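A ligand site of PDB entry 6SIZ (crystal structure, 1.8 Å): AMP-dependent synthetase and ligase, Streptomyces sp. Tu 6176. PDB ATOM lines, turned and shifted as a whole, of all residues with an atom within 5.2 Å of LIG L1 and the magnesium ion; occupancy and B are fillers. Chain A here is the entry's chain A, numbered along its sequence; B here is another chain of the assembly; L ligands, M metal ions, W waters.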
ATOM      1  N   LYS A  63      -0.647 -21.328  26.860  1.00  0.00           N
ATOM      2  CA  LYS A  63      -1.081 -21.524  25.454  1.00  0.00           C
ATOM      3  C   LYS A  63      -2.555 -21.138  25.294  1.00  0.00           C
ATOM      4  O   LYS A  63      -2.889 -20.508  24.276  1.00  0.00           O
ATOM      5  CB  LYS A  63      -0.965 -22.992  25.047  1.00  0.00           C
ATOM      6  CG  LYS A  63       0.394 -23.472  24.567  1.00  0.00           C
ATOM      7  CD  LYS A  63       0.285 -24.826  23.884  1.00  0.00           C
ATOM      8  CE  LYS A  63       1.612 -25.531  23.735  1.00  0.00           C
ATOM      9  NZ  LYS A  63       2.574 -24.700  22.960  1.00  0.00           N
ATOM     10  N   ARG A  67      -4.662 -18.716  22.587  1.00  0.00           N
ATOM     11  CA  ARG A  67      -5.801 -19.181  21.767  1.00  0.00           C
ATOM     12  C   ARG A  67      -7.030 -18.295  22.046  1.00  0.00           C
ATOM     13  O   ARG A  67      -7.707 -17.922  21.071  1.00  0.00           O
ATOM     14  CB  ARG A  67      -6.126 -20.653  22.033  1.00  0.00           C
ATOM     15  CG  ARG A  67      -5.013 -21.615  21.637  1.00  0.00           C
ATOM     16  CD  ARG A  67      -5.477 -23.040  21.847  1.00  0.00           C
ATOM     17  NE  ARG A  67      -4.403 -24.002  21.576  1.00  0.00           N
ATOM     18  CZ  ARG A  67      -3.913 -24.879  22.445  1.00  0.00           C
ATOM     19  NH1 ARG A  67      -4.398 -24.955  23.677  1.00  0.00           N
ATOM     20  NH2 ARG A  67      -2.934 -25.683  22.072  1.00  0.00           N
ATOM     21  N   SER A  88       0.431 -21.563  14.509  1.00  0.00           N
ATOM     22  CA  SER A  88       1.130 -22.768  14.993  1.00  0.00           C
ATOM     23  C   SER A  88       0.639 -24.002  14.238  1.00  0.00           C
ATOM     24  O   SER A  88      -0.495 -23.949  13.703  1.00  0.00           O
ATOM     25  CB  SER A  88       0.942 -22.935  16.462  1.00  0.00           C
ATOM     26  OG  SER A  88       1.620 -21.896  17.139  1.00  0.00           O
ATOM     27  N   SER A  89       1.455 -25.053  14.225  1.00  0.00           N
ATOM     28  CA  SER A  89       1.051 -26.432  13.882  1.00  0.00           C
ATOM     29  C   SER A  89       0.102 -26.939  14.979  1.00  0.00           C
ATOM     30  O   SER A  89      -0.182 -26.168  15.923  1.00  0.00           O
ATOM     31  CB  SER A  89       2.266 -27.292  13.691  1.00  0.00           C
ATOM     32  OG  SER A  89       2.955 -27.443  14.919  1.00  0.00           O
ATOM     33  N   GLY A  90      -0.406 -28.169  14.854  1.00  0.00           N
ATOM     34  CA  GLY A  90      -1.387 -28.748  15.795  1.00  0.00           C
ATOM     35  C   GLY A  90      -2.827 -28.481  15.362  1.00  0.00           C
ATOM     36  O   GLY A  90      -3.068 -28.449  14.138  1.00  0.00           O
ATOM     37  N   THR A  91      -3.748 -28.311  16.324  1.00  0.00           N
ATOM     38  CA  THR A  91      -5.222 -28.261  16.100  1.00  0.00           C
ATOM     39  C   THR A  91      -5.555 -27.075  15.195  1.00  0.00           C
ATOM     40  O   THR A  91      -5.120 -25.956  15.521  1.00  0.00           O
ATOM     41  CB  THR A  91      -5.994 -28.174  17.422  1.00  0.00           C
ATOM     42  OG1 THR A  91      -5.551 -29.238  18.266  1.00  0.00           O
ATOM     43  CG2 THR A  91      -7.498 -28.277  17.248  1.00  0.00           C
ATOM     44  N   THR A  96      -3.512 -20.585  17.016  1.00  0.00           N
ATOM     45  CA  THR A  96      -2.609 -19.728  17.813  1.00  0.00           C
ATOM     46  C   THR A  96      -1.863 -18.829  16.823  1.00  0.00           C
ATOM     47  O   THR A  96      -1.144 -19.368  15.980  1.00  0.00           O
ATOM     48  CB  THR A  96      -1.641 -20.540  18.680  1.00  0.00           C
ATOM     49  OG1 THR A  96      -2.418 -21.379  19.533  1.00  0.00           O
ATOM     50  CG2 THR A  96      -0.750 -19.651  19.515  1.00  0.00           C
ATOM     51  N   ALA A 212      14.828 -30.122  13.767  1.00  0.00           N
ATOM     52  CA  ALA A 212      14.030 -29.688  14.923  1.00  0.00           C
ATOM     53  C   ALA A 212      12.641 -30.302  14.805  1.00  0.00           C
ATOM     54  O   ALA A 212      12.413 -31.053  13.819  1.00  0.00           O
ATOM     55  CB  ALA A 212      13.945 -28.178  14.945  1.00  0.00           C
ATOM     56  N   ALA A 213      11.752 -29.941  15.711  1.00  0.00           N
ATOM     57  CA  ALA A 213      10.270 -30.097  15.618  1.00  0.00           C
ATOM     58  C   ALA A 213       9.812 -31.485  16.085  1.00  0.00           C
ATOM     59  O   ALA A 213       8.603 -31.770  15.942  1.00  0.00           O
ATOM     60  CB  ALA A 213       9.803 -29.832  14.213  1.00  0.00           C
ATOM     61  N   GLU A 214      10.708 -32.351  16.547  1.00  0.00           N
ATOM     62  CA  GLU A 214      10.302 -33.570  17.296  1.00  0.00           C
ATOM     63  C   GLU A 214      11.353 -33.966  18.317  1.00  0.00           C
ATOM     64  O   GLU A 214      12.538 -33.704  18.178  1.00  0.00           O
ATOM     65  CB  GLU A 214       9.860 -34.745  16.416  1.00  0.00           C
ATOM     66  CG  GLU A 214      10.663 -35.035  15.180  1.00  0.00           C
ATOM     67  CD  GLU A 214      10.190 -36.251  14.377  1.00  0.00           C
ATOM     68  OE1 GLU A 214       9.932 -36.098  13.170  1.00  0.00           O
ATOM     69  OE2 GLU A 214      10.306 -37.376  14.905  1.00  0.00           O
ATOM     70  N   PRO A 215      10.907 -34.623  19.408  1.00  0.00           N
ATOM     71  CA  PRO A 215      11.817 -35.190  20.405  1.00  0.00           C
ATOM     72  C   PRO A 215      12.797 -36.124  19.692  1.00  0.00           C
ATOM     73  O   PRO A 215      12.361 -36.961  18.912  1.00  0.00           O
ATOM     74  CB  PRO A 215      10.887 -35.969  21.344  1.00  0.00           C
ATOM     75  CG  PRO A 215       9.544 -35.278  21.198  1.00  0.00           C
ATOM     76  CD  PRO A 215       9.493 -34.839  19.749  1.00  0.00           C
ATOM     77  N   LEU A 216      14.082 -35.918  19.893  1.00  0.00           N
ATOM     78  CA  LEU A 216      15.150 -36.621  19.141  1.00  0.00           C
ATOM     79  C   LEU A 216      16.192 -37.151  20.128  1.00  0.00           C
ATOM     80  O   LEU A 216      16.900 -36.326  20.742  1.00  0.00           O
ATOM     81  CB  LEU A 216      15.753 -35.654  18.108  1.00  0.00           C
ATOM     82  CG  LEU A 216      16.861 -36.249  17.251  1.00  0.00           C
ATOM     83  CD1 LEU A 216      16.370 -37.459  16.473  1.00  0.00           C
ATOM     84  CD2 LEU A 216      17.432 -35.209  16.311  1.00  0.00           C
ATOM     85  N   GLU A 235      20.773 -30.067  15.740  1.00  0.00           N
ATOM     86  CA  GLU A 235      19.422 -29.904  16.292  1.00  0.00           C
ATOM     87  C   GLU A 235      19.244 -28.472  16.809  1.00  0.00           C
ATOM     88  O   GLU A 235      20.229 -27.889  17.322  1.00  0.00           O
ATOM     89  CB  GLU A 235      19.202 -30.903  17.426  1.00  0.00           C
ATOM     90  CG  GLU A 235      17.747 -31.022  17.823  1.00  0.00           C
ATOM     91  CD  GLU A 235      17.490 -31.984  18.983  1.00  0.00           C
ATOM     92  OE1 GLU A 235      18.482 -32.525  19.553  1.00  0.00           O
ATOM     93  OE2 GLU A 235      16.308 -32.155  19.327  1.00  0.00           O
ATOM     94  N   GLU A 236      18.040 -27.954  16.672  1.00  0.00           N
ATOM     95  CA  GLU A 236      17.592 -26.765  17.444  1.00  0.00           C
ATOM     96  C   GLU A 236      16.200 -27.076  17.994  1.00  0.00           C
ATOM     97  O   GLU A 236      15.589 -28.066  17.605  1.00  0.00           O
ATOM     98  CB  GLU A 236      17.658 -25.475  16.616  1.00  0.00           C
ATOM     99  CG  GLU A 236      16.557 -25.323  15.586  1.00  0.00           C
ATOM    100  CD  GLU A 236      16.332 -23.910  15.100  1.00  0.00           C
ATOM    101  OE1 GLU A 236      17.282 -23.328  14.511  1.00  0.00           O
ATOM    102  OE2 GLU A 236      15.234 -23.368  15.338  1.00  0.00           O
ATOM    103  N   TYR A 237      15.759 -26.210  18.888  1.00  0.00           N
ATOM    104  CA  TYR A 237      14.480 -26.261  19.632  1.00  0.00           C
ATOM    105  C   TYR A 237      13.854 -24.880  19.517  1.00  0.00           C
ATOM    106  O   TYR A 237      14.577 -23.894  19.777  1.00  0.00           O
ATOM    107  CB  TYR A 237      14.741 -26.731  21.050  1.00  0.00           C
ATOM    108  CG  TYR A 237      13.581 -26.614  22.022  1.00  0.00           C
ATOM    109  CD1 TYR A 237      12.277 -26.912  21.645  1.00  0.00           C
ATOM    110  CD2 TYR A 237      13.802 -26.245  23.341  1.00  0.00           C
ATOM    111  CE1 TYR A 237      11.231 -26.817  22.555  1.00  0.00           C
ATOM    112  CE2 TYR A 237      12.768 -26.149  24.244  1.00  0.00           C
ATOM    113  CZ  TYR A 237      11.473 -26.438  23.855  1.00  0.00           C
ATOM    114  OH  TYR A 237      10.448 -26.337  24.759  1.00  0.00           O
ATOM    115  N   GLY A 238      12.606 -24.808  19.057  1.00  0.00           N
ATOM    116  CA  GLY A 238      11.872 -23.542  18.859  1.00  0.00           C
ATOM    117  C   GLY A 238      10.370 -23.727  18.891  1.00  0.00           C
ATOM    118  O   GLY A 238       9.914 -24.865  19.049  1.00  0.00           O
ATOM    119  N   SER A 239       9.640 -22.617  18.770  1.00  0.00           N
ATOM    120  CA  SER A 239       8.170 -22.581  18.579  1.00  0.00           C
ATOM    121  C   SER A 239       7.817 -21.367  17.711  1.00  0.00           C
ATOM    122  O   SER A 239       8.660 -20.446  17.577  1.00  0.00           O
ATOM    123  CB  SER A 239       7.437 -22.556  19.898  1.00  0.00           C
ATOM    124  OG  SER A 239       7.518 -21.281  20.525  1.00  0.00           O
ATOM    125  N   THR A 240       6.624 -21.381  17.124  1.00  0.00           N
ATOM    126  CA  THR A 240       6.089 -20.252  16.329  1.00  0.00           C
ATOM    127  C   THR A 240       6.031 -18.984  17.187  1.00  0.00           C
ATOM    128  O   THR A 240       6.315 -17.878  16.654  1.00  0.00           O
ATOM    129  CB  THR A 240       4.731 -20.614  15.748  1.00  0.00           C
ATOM    130  OG1 THR A 240       4.854 -21.944  15.267  1.00  0.00           O
ATOM    131  CG2 THR A 240       4.308 -19.652  14.665  1.00  0.00           C
ATOM    132  N   GLU A 241       5.687 -19.128  18.463  1.00  0.00           N
ATOM    133  CA  GLU A 241       5.454 -18.018  19.418  1.00  0.00           C
ATOM    134  C   GLU A 241       6.771 -17.417  19.915  1.00  0.00           C
ATOM    135  O   GLU A 241       6.720 -16.263  20.393  1.00  0.00           O
ATOM    136  CB  GLU A 241       4.651 -18.498  20.633  1.00  0.00           C
ATOM    137  CG  GLU A 241       3.272 -19.046  20.298  1.00  0.00           C
ATOM    138  CD  GLU A 241       3.250 -20.444  19.695  1.00  0.00           C
ATOM    139  OE1 GLU A 241       2.277 -20.758  18.987  1.00  0.00           O
ATOM    140  OE2 GLU A 241       4.201 -21.206  19.940  1.00  0.00           O
ATOM    141  N   MET A 254      22.070 -29.261  23.197  1.00  0.00           N
ATOM    142  CA  MET A 254      21.375 -27.998  22.887  1.00  0.00           C
ATOM    143  C   MET A 254      21.575 -27.024  24.061  1.00  0.00           C
ATOM    144  O   MET A 254      21.281 -27.415  25.192  1.00  0.00           O
ATOM    145  CB  MET A 254      19.886 -28.206  22.627  1.00  0.00           C
ATOM    146  CG  MET A 254      19.618 -28.906  21.306  1.00  0.00           C
ATOM    147  SD  MET A 254      17.881 -28.786  20.752  1.00  0.00           S
ATOM    148  CE  MET A 254      17.062 -29.735  22.031  1.00  0.00           C
ATOM    149  N   TYR A 296       5.826 -17.223  29.126  1.00  0.00           N
ATOM    150  CA  TYR A 296       4.984 -18.067  28.243  1.00  0.00           C
ATOM    151  C   TYR A 296       5.401 -19.528  28.440  1.00  0.00           C
ATOM    152  O   TYR A 296       6.572 -19.894  28.171  1.00  0.00           O
ATOM    153  CB  TYR A 296       5.073 -17.607  26.794  1.00  0.00           C
ATOM    154  CG  TYR A 296       4.465 -18.588  25.823  1.00  0.00           C
ATOM    155  CD1 TYR A 296       3.110 -18.838  25.840  1.00  0.00           C
ATOM    156  CD2 TYR A 296       5.251 -19.281  24.916  1.00  0.00           C
ATOM    157  CE1 TYR A 296       2.543 -19.749  24.958  1.00  0.00           C
ATOM    158  CE2 TYR A 296       4.701 -20.181  24.036  1.00  0.00           C
ATOM    159  CZ  TYR A 296       3.343 -20.428  24.061  1.00  0.00           C
ATOM    160  OH  TYR A 296       2.817 -21.333  23.194  1.00  0.00           O
ATOM    161  N   LEU A 298       5.454 -23.034  27.189  1.00  0.00           N
ATOM    162  CA  LEU A 298       5.392 -23.923  25.994  1.00  0.00           C
ATOM    163  C   LEU A 298       4.708 -25.248  26.362  1.00  0.00           C
ATOM    164  O   LEU A 298       4.252 -25.945  25.435  1.00  0.00           O
ATOM    165  CB  LEU A 298       6.805 -24.196  25.484  1.00  0.00           C
ATOM    166  CG  LEU A 298       7.362 -23.197  24.476  1.00  0.00           C
ATOM    167  CD1 LEU A 298       6.555 -23.227  23.192  1.00  0.00           C
ATOM    168  CD2 LEU A 298       7.412 -21.804  25.069  1.00  0.00           C
ATOM    169  N   ASP A 300       6.143 -27.835  27.125  1.00  0.00           N
ATOM    170  CA  ASP A 300       7.088 -28.915  26.763  1.00  0.00           C
ATOM    171  C   ASP A 300       7.800 -29.382  28.034  1.00  0.00           C
ATOM    172  O   ASP A 300       8.296 -28.526  28.795  1.00  0.00           O
ATOM    173  CB  ASP A 300       8.146 -28.452  25.768  1.00  0.00           C
ATOM    174  CG  ASP A 300       7.632 -28.152  24.374  1.00  0.00           C
ATOM    175  OD1 ASP A 300       6.701 -28.853  23.917  1.00  0.00           O
ATOM    176  OD2 ASP A 300       8.194 -27.248  23.721  1.00  0.00           O
ATOM    177  N   VAL A 320      14.742 -31.967  25.523  1.00  0.00           N
ATOM    178  CA  VAL A 320      13.272 -31.826  25.293  1.00  0.00           C
ATOM    179  C   VAL A 320      12.676 -33.229  25.215  1.00  0.00           C
ATOM    180  O   VAL A 320      12.847 -33.894  24.185  1.00  0.00           O
ATOM    181  CB  VAL A 320      12.986 -30.978  24.038  1.00  0.00           C
ATOM    182  CG1 VAL A 320      11.508 -30.632  23.919  1.00  0.00           C
ATOM    183  CG2 VAL A 320      13.836 -29.722  24.018  1.00  0.00           C
ATOM    184  N   LYS B 419       2.562 -33.766  13.406  1.00  0.00           N
ATOM    185  CA  LYS B 419       4.008 -34.086  13.358  1.00  0.00           C
ATOM    186  C   LYS B 419       4.164 -35.588  13.598  1.00  0.00           C
ATOM    187  O   LYS B 419       3.213 -36.186  14.183  1.00  0.00           O
ATOM    188  CB  LYS B 419       4.763 -33.265  14.407  1.00  0.00           C
ATOM    189  CG  LYS B 419       4.600 -31.768  14.261  1.00  0.00           C
ATOM    190  CD  LYS B 419       5.409 -30.992  15.282  1.00  0.00           C
ATOM    191  CE  LYS B 419       4.783 -29.661  15.629  1.00  0.00           C
ATOM    192  NZ  LYS B 419       5.314 -29.133  16.904  1.00  0.00           N
HETATM  193  P1  LIG L   1       0.238 -25.869  19.933  1.00  0.00           P
HETATM  194  O1  LIG L   1       0.913 -24.657  20.537  1.00  0.00           O
HETATM  195  O2  LIG L   1      -1.185 -25.509  19.582  1.00  0.00           O
HETATM  196  O3  LIG L   1       0.251 -27.011  20.935  1.00  0.00           O
HETATM  197  P2  LIG L   1       2.655 -26.748  18.611  1.00  0.00           P
HETATM  198  O4  LIG L   1       3.106 -27.085  20.020  1.00  0.00           O
HETATM  199  O5  LIG L   1       2.929 -27.721  17.499  1.00  0.00           O
HETATM  200  N1  LIG L   1       1.081 -26.306  18.608  1.00  0.00           N
HETATM  201  P3  LIG L   1       4.556 -25.025  17.130  1.00  0.00           P
HETATM  202  O6  LIG L   1       5.051 -23.670  17.522  1.00  0.00           O
HETATM  203  O7  LIG L   1       3.957 -25.231  15.779  1.00  0.00           O
HETATM  204  O8  LIG L   1       3.451 -25.394  18.239  1.00  0.00           O
HETATM  205  O9  LIG L   1       5.694 -26.134  17.382  1.00  0.00           O
HETATM  206  C1  LIG L   1       6.722 -25.950  18.398  1.00  0.00           C
HETATM  207  C2  LIG L   1       6.855 -27.203  19.242  1.00  0.00           C
HETATM  208  O10 LIG L   1       7.541 -28.251  18.512  1.00  0.00           O
HETATM  209  C3  LIG L   1       7.685 -27.051  20.512  1.00  0.00           C
HETATM  210  O11 LIG L   1       6.981 -26.424  21.567  1.00  0.00           O
HETATM  211  C4  LIG L   1       7.952 -28.521  20.830  1.00  0.00           C
HETATM  212  O12 LIG L   1       6.814 -29.182  21.332  1.00  0.00           O
HETATM  213  C5  LIG L   1       8.276 -29.038  19.437  1.00  0.00           C
HETATM  214  N2  LIG L   1       9.719 -28.961  19.162  1.00  0.00           N
HETATM  215  C6  LIG L   1      10.400 -28.100  18.318  1.00  0.00           C
HETATM  216  N3  LIG L   1      11.694 -28.361  18.261  1.00  0.00           N
HETATM  217  C7  LIG L   1      11.862 -29.475  19.089  1.00  0.00           C
HETATM  218  C8  LIG L   1      12.978 -30.257  19.446  1.00  0.00           C
HETATM  219  N4  LIG L   1      14.218 -30.043  18.987  1.00  0.00           N
HETATM  220  N5  LIG L   1      12.776 -31.321  20.264  1.00  0.00           N
HETATM  221  C9  LIG L   1      11.540 -31.543  20.729  1.00  0.00           C
HETATM  222  N6  LIG L   1      10.418 -30.885  20.464  1.00  0.00           N
HETATM  223  C10 LIG L   1      10.646 -29.860  19.628  1.00  0.00           C
HETATM  224  O1  LG2 L   2       8.538 -26.285  14.856  1.00  0.00           O
HETATM  225  C1  LG2 L   2       8.408 -25.069  15.083  1.00  0.00           C
HETATM  226  O2  LG2 L   2       7.303 -24.542  15.361  1.00  0.00           O
HETATM  227  C2  LG2 L   2       9.655 -24.245  15.114  1.00  0.00           C
HETATM  228  C3  LG2 L   2       9.666 -22.862  14.881  1.00  0.00           C
HETATM  229  C4  LG2 L   2      10.861 -22.154  14.957  1.00  0.00           C
HETATM  230  C5  LG2 L   2      12.084 -22.770  15.244  1.00  0.00           C
HETATM  231  C6  LG2 L   2      12.144 -24.132  15.472  1.00  0.00           C
HETATM  232  O3  LG2 L   2      13.288 -24.778  15.776  1.00  0.00           O
HETATM  233  C7  LG2 L   2      10.908 -24.935  15.424  1.00  0.00           C
HETATM  234  N1  LG2 L   2      10.932 -26.276  15.651  1.00  0.00           N
HETATM  235 MG    MG M   1       2.759 -23.500  19.353  1.00  0.00          MG
HETATM  236  O   HOH W   1       8.038 -31.933  21.638  1.00  0.00           O
HETATM  237  O   HOH W   2      14.398 -32.447  16.763  1.00  0.00           O
HETATM  238  O   HOH W   3      14.683 -33.082  21.153  1.00  0.00           O
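The backbone NH (N) of Ser 89 is in hydrogen-bond range of an oxygen (O7) of LIG L1 (3.0 Å). OE2 of Glu 235 lies within hydrogen-bond range of N4 of LIG L1. The side-chain amino group of Lys 63 lies within salt-bridge range of an oxygen (O4) of LIG L1 (3.8 Å). OE2 of Glu 236 is in hydrogen-bond range of O3 of LG2 L2 (2.4 Å). An oxygen (O7) of LIG L1 lies within hydrogen-bond range of the side-chain hydroxyl (OG) of Ser 89 (2.6 Å). The side-chain carboxylate (OD2) of Asp 300 is in hydrogen-bond range of an oxygen (O11) of LIG L1, at 2.6 Å. O of Glu 236 is in hydrogen-bond range of N4 of LIG L1, 2.8 Å away. NH2 of Arg 67 lies within salt-bridge range of O2 of LIG L1 (3.0 Å). A nitrogen (N3) of LIG L1 lies within hydrogen-bond range of the backbone NH (N) of Ala 213 (3.0 Å). The backbone NH of Thr 240 lies within hydrogen-bond range of an oxygen (O6) of LIG L1 (2.8 Å). O3 of LG2 L2 sits at hydrogen-bond distance from N of Gly 238. An oxygen (O5) of LIG L1 lies within salt-bridge range of the side-chain amino group (NZ) of Lys 419 of chain B (2.8 Å). The side-chain hydroxyl (OG1) of Thr 240 lies within hydrogen-bond range of an oxygen (O6) of LIG L1 (2.8 Å). The backbone carbonyl oxygen (O) of Ser 89 lies within hydrogen-bond range of a nitrogen (N1) of LIG L1 (3.0 Å).
A nitrogen (N3) of LIG L1 lies close to a nitrogen (N1) of LG2 L2 (3.4 Å).
The side-chain amino group (NZ) of Lys 63 sits close to the backbone carbonyl oxygen (O) of Leu 298 (3.2 Å). The backbone NH of Ser 88 sits at hydrogen-bond distance from the backbone carbonyl oxygen of Thr 96, 3.1 Å away. The side-chain carboxylate (OE2) of Glu 241 sits at hydrogen-bond distance from the side-chain hydroxyl (OG) of Ser 239. The side-chain hydroxyl (OH) of Tyr 296 is in hydrogen-bond range of the side-chain amino group (NZ) of Lys 63. OD2 of Asp 300 lies within hydrogen-bond range of OH of Tyr 237, at 2.6 Å.
A nitrogen (N5) of LIG L1 sits close to the backbone carbonyl oxygen of Glu 214, 3.2 Å away. Ser 88 touches LIG L1. Pro 215 touches LIG L1. Tyr 237 touches LIG L1. O of Gly 238 touches C6 of LIG L1 (3.4 Å). Ser 239 touches LIG L1 (CA to O6, 3.5 Å). CD1 of Leu 298 touches O11 of LIG L1, at 3.6 Å. CG1 of Val 320 touches C9 of LIG L1 (3.3 Å). Hydrophobic or aromatic side chains within 4 Å of LIG L1: Tyr 237, Leu 298 and Val 320. Of the 25 residues printed, 18 come within 4 Å of LIG L1.
Residues that only touch the magnesium ion: Ser 88 (3.0 Å) and Lys 63 (3.8 Å). Three residues have an atom within 4 Å of the magnesium ion: Lys 63, Ser 88 and Glu 241. The nearest printed residue that does not touch the magnesium ion is Tyr 296 (4.4 Å).
The magnesium ion is bound by an oxygen (O8) of LIG L1 (2.3 Å) and an oxygen (O1) of LIG L1 (2.5 Å). Slightly farther from the magnesium ion lies OE2 of Glu 241 (2.8 Å). Slightly farther from the magnesium ion lies the side-chain carboxylate (OE1) of Glu 241 (2.8 Å).
Water W3 lies within hydrogen-bond range of the side-chain carboxylate (OE2) of Glu 235, a nitrogen (N5) of LIG L1 and the backbone NH (N) of Leu 216. Water W2 lies within hydrogen-bond range of O of Glu 214 (2.7 Å), OE2 of Glu 235 (3.2 Å) and N4 of LIG L1 (3.3 Å).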
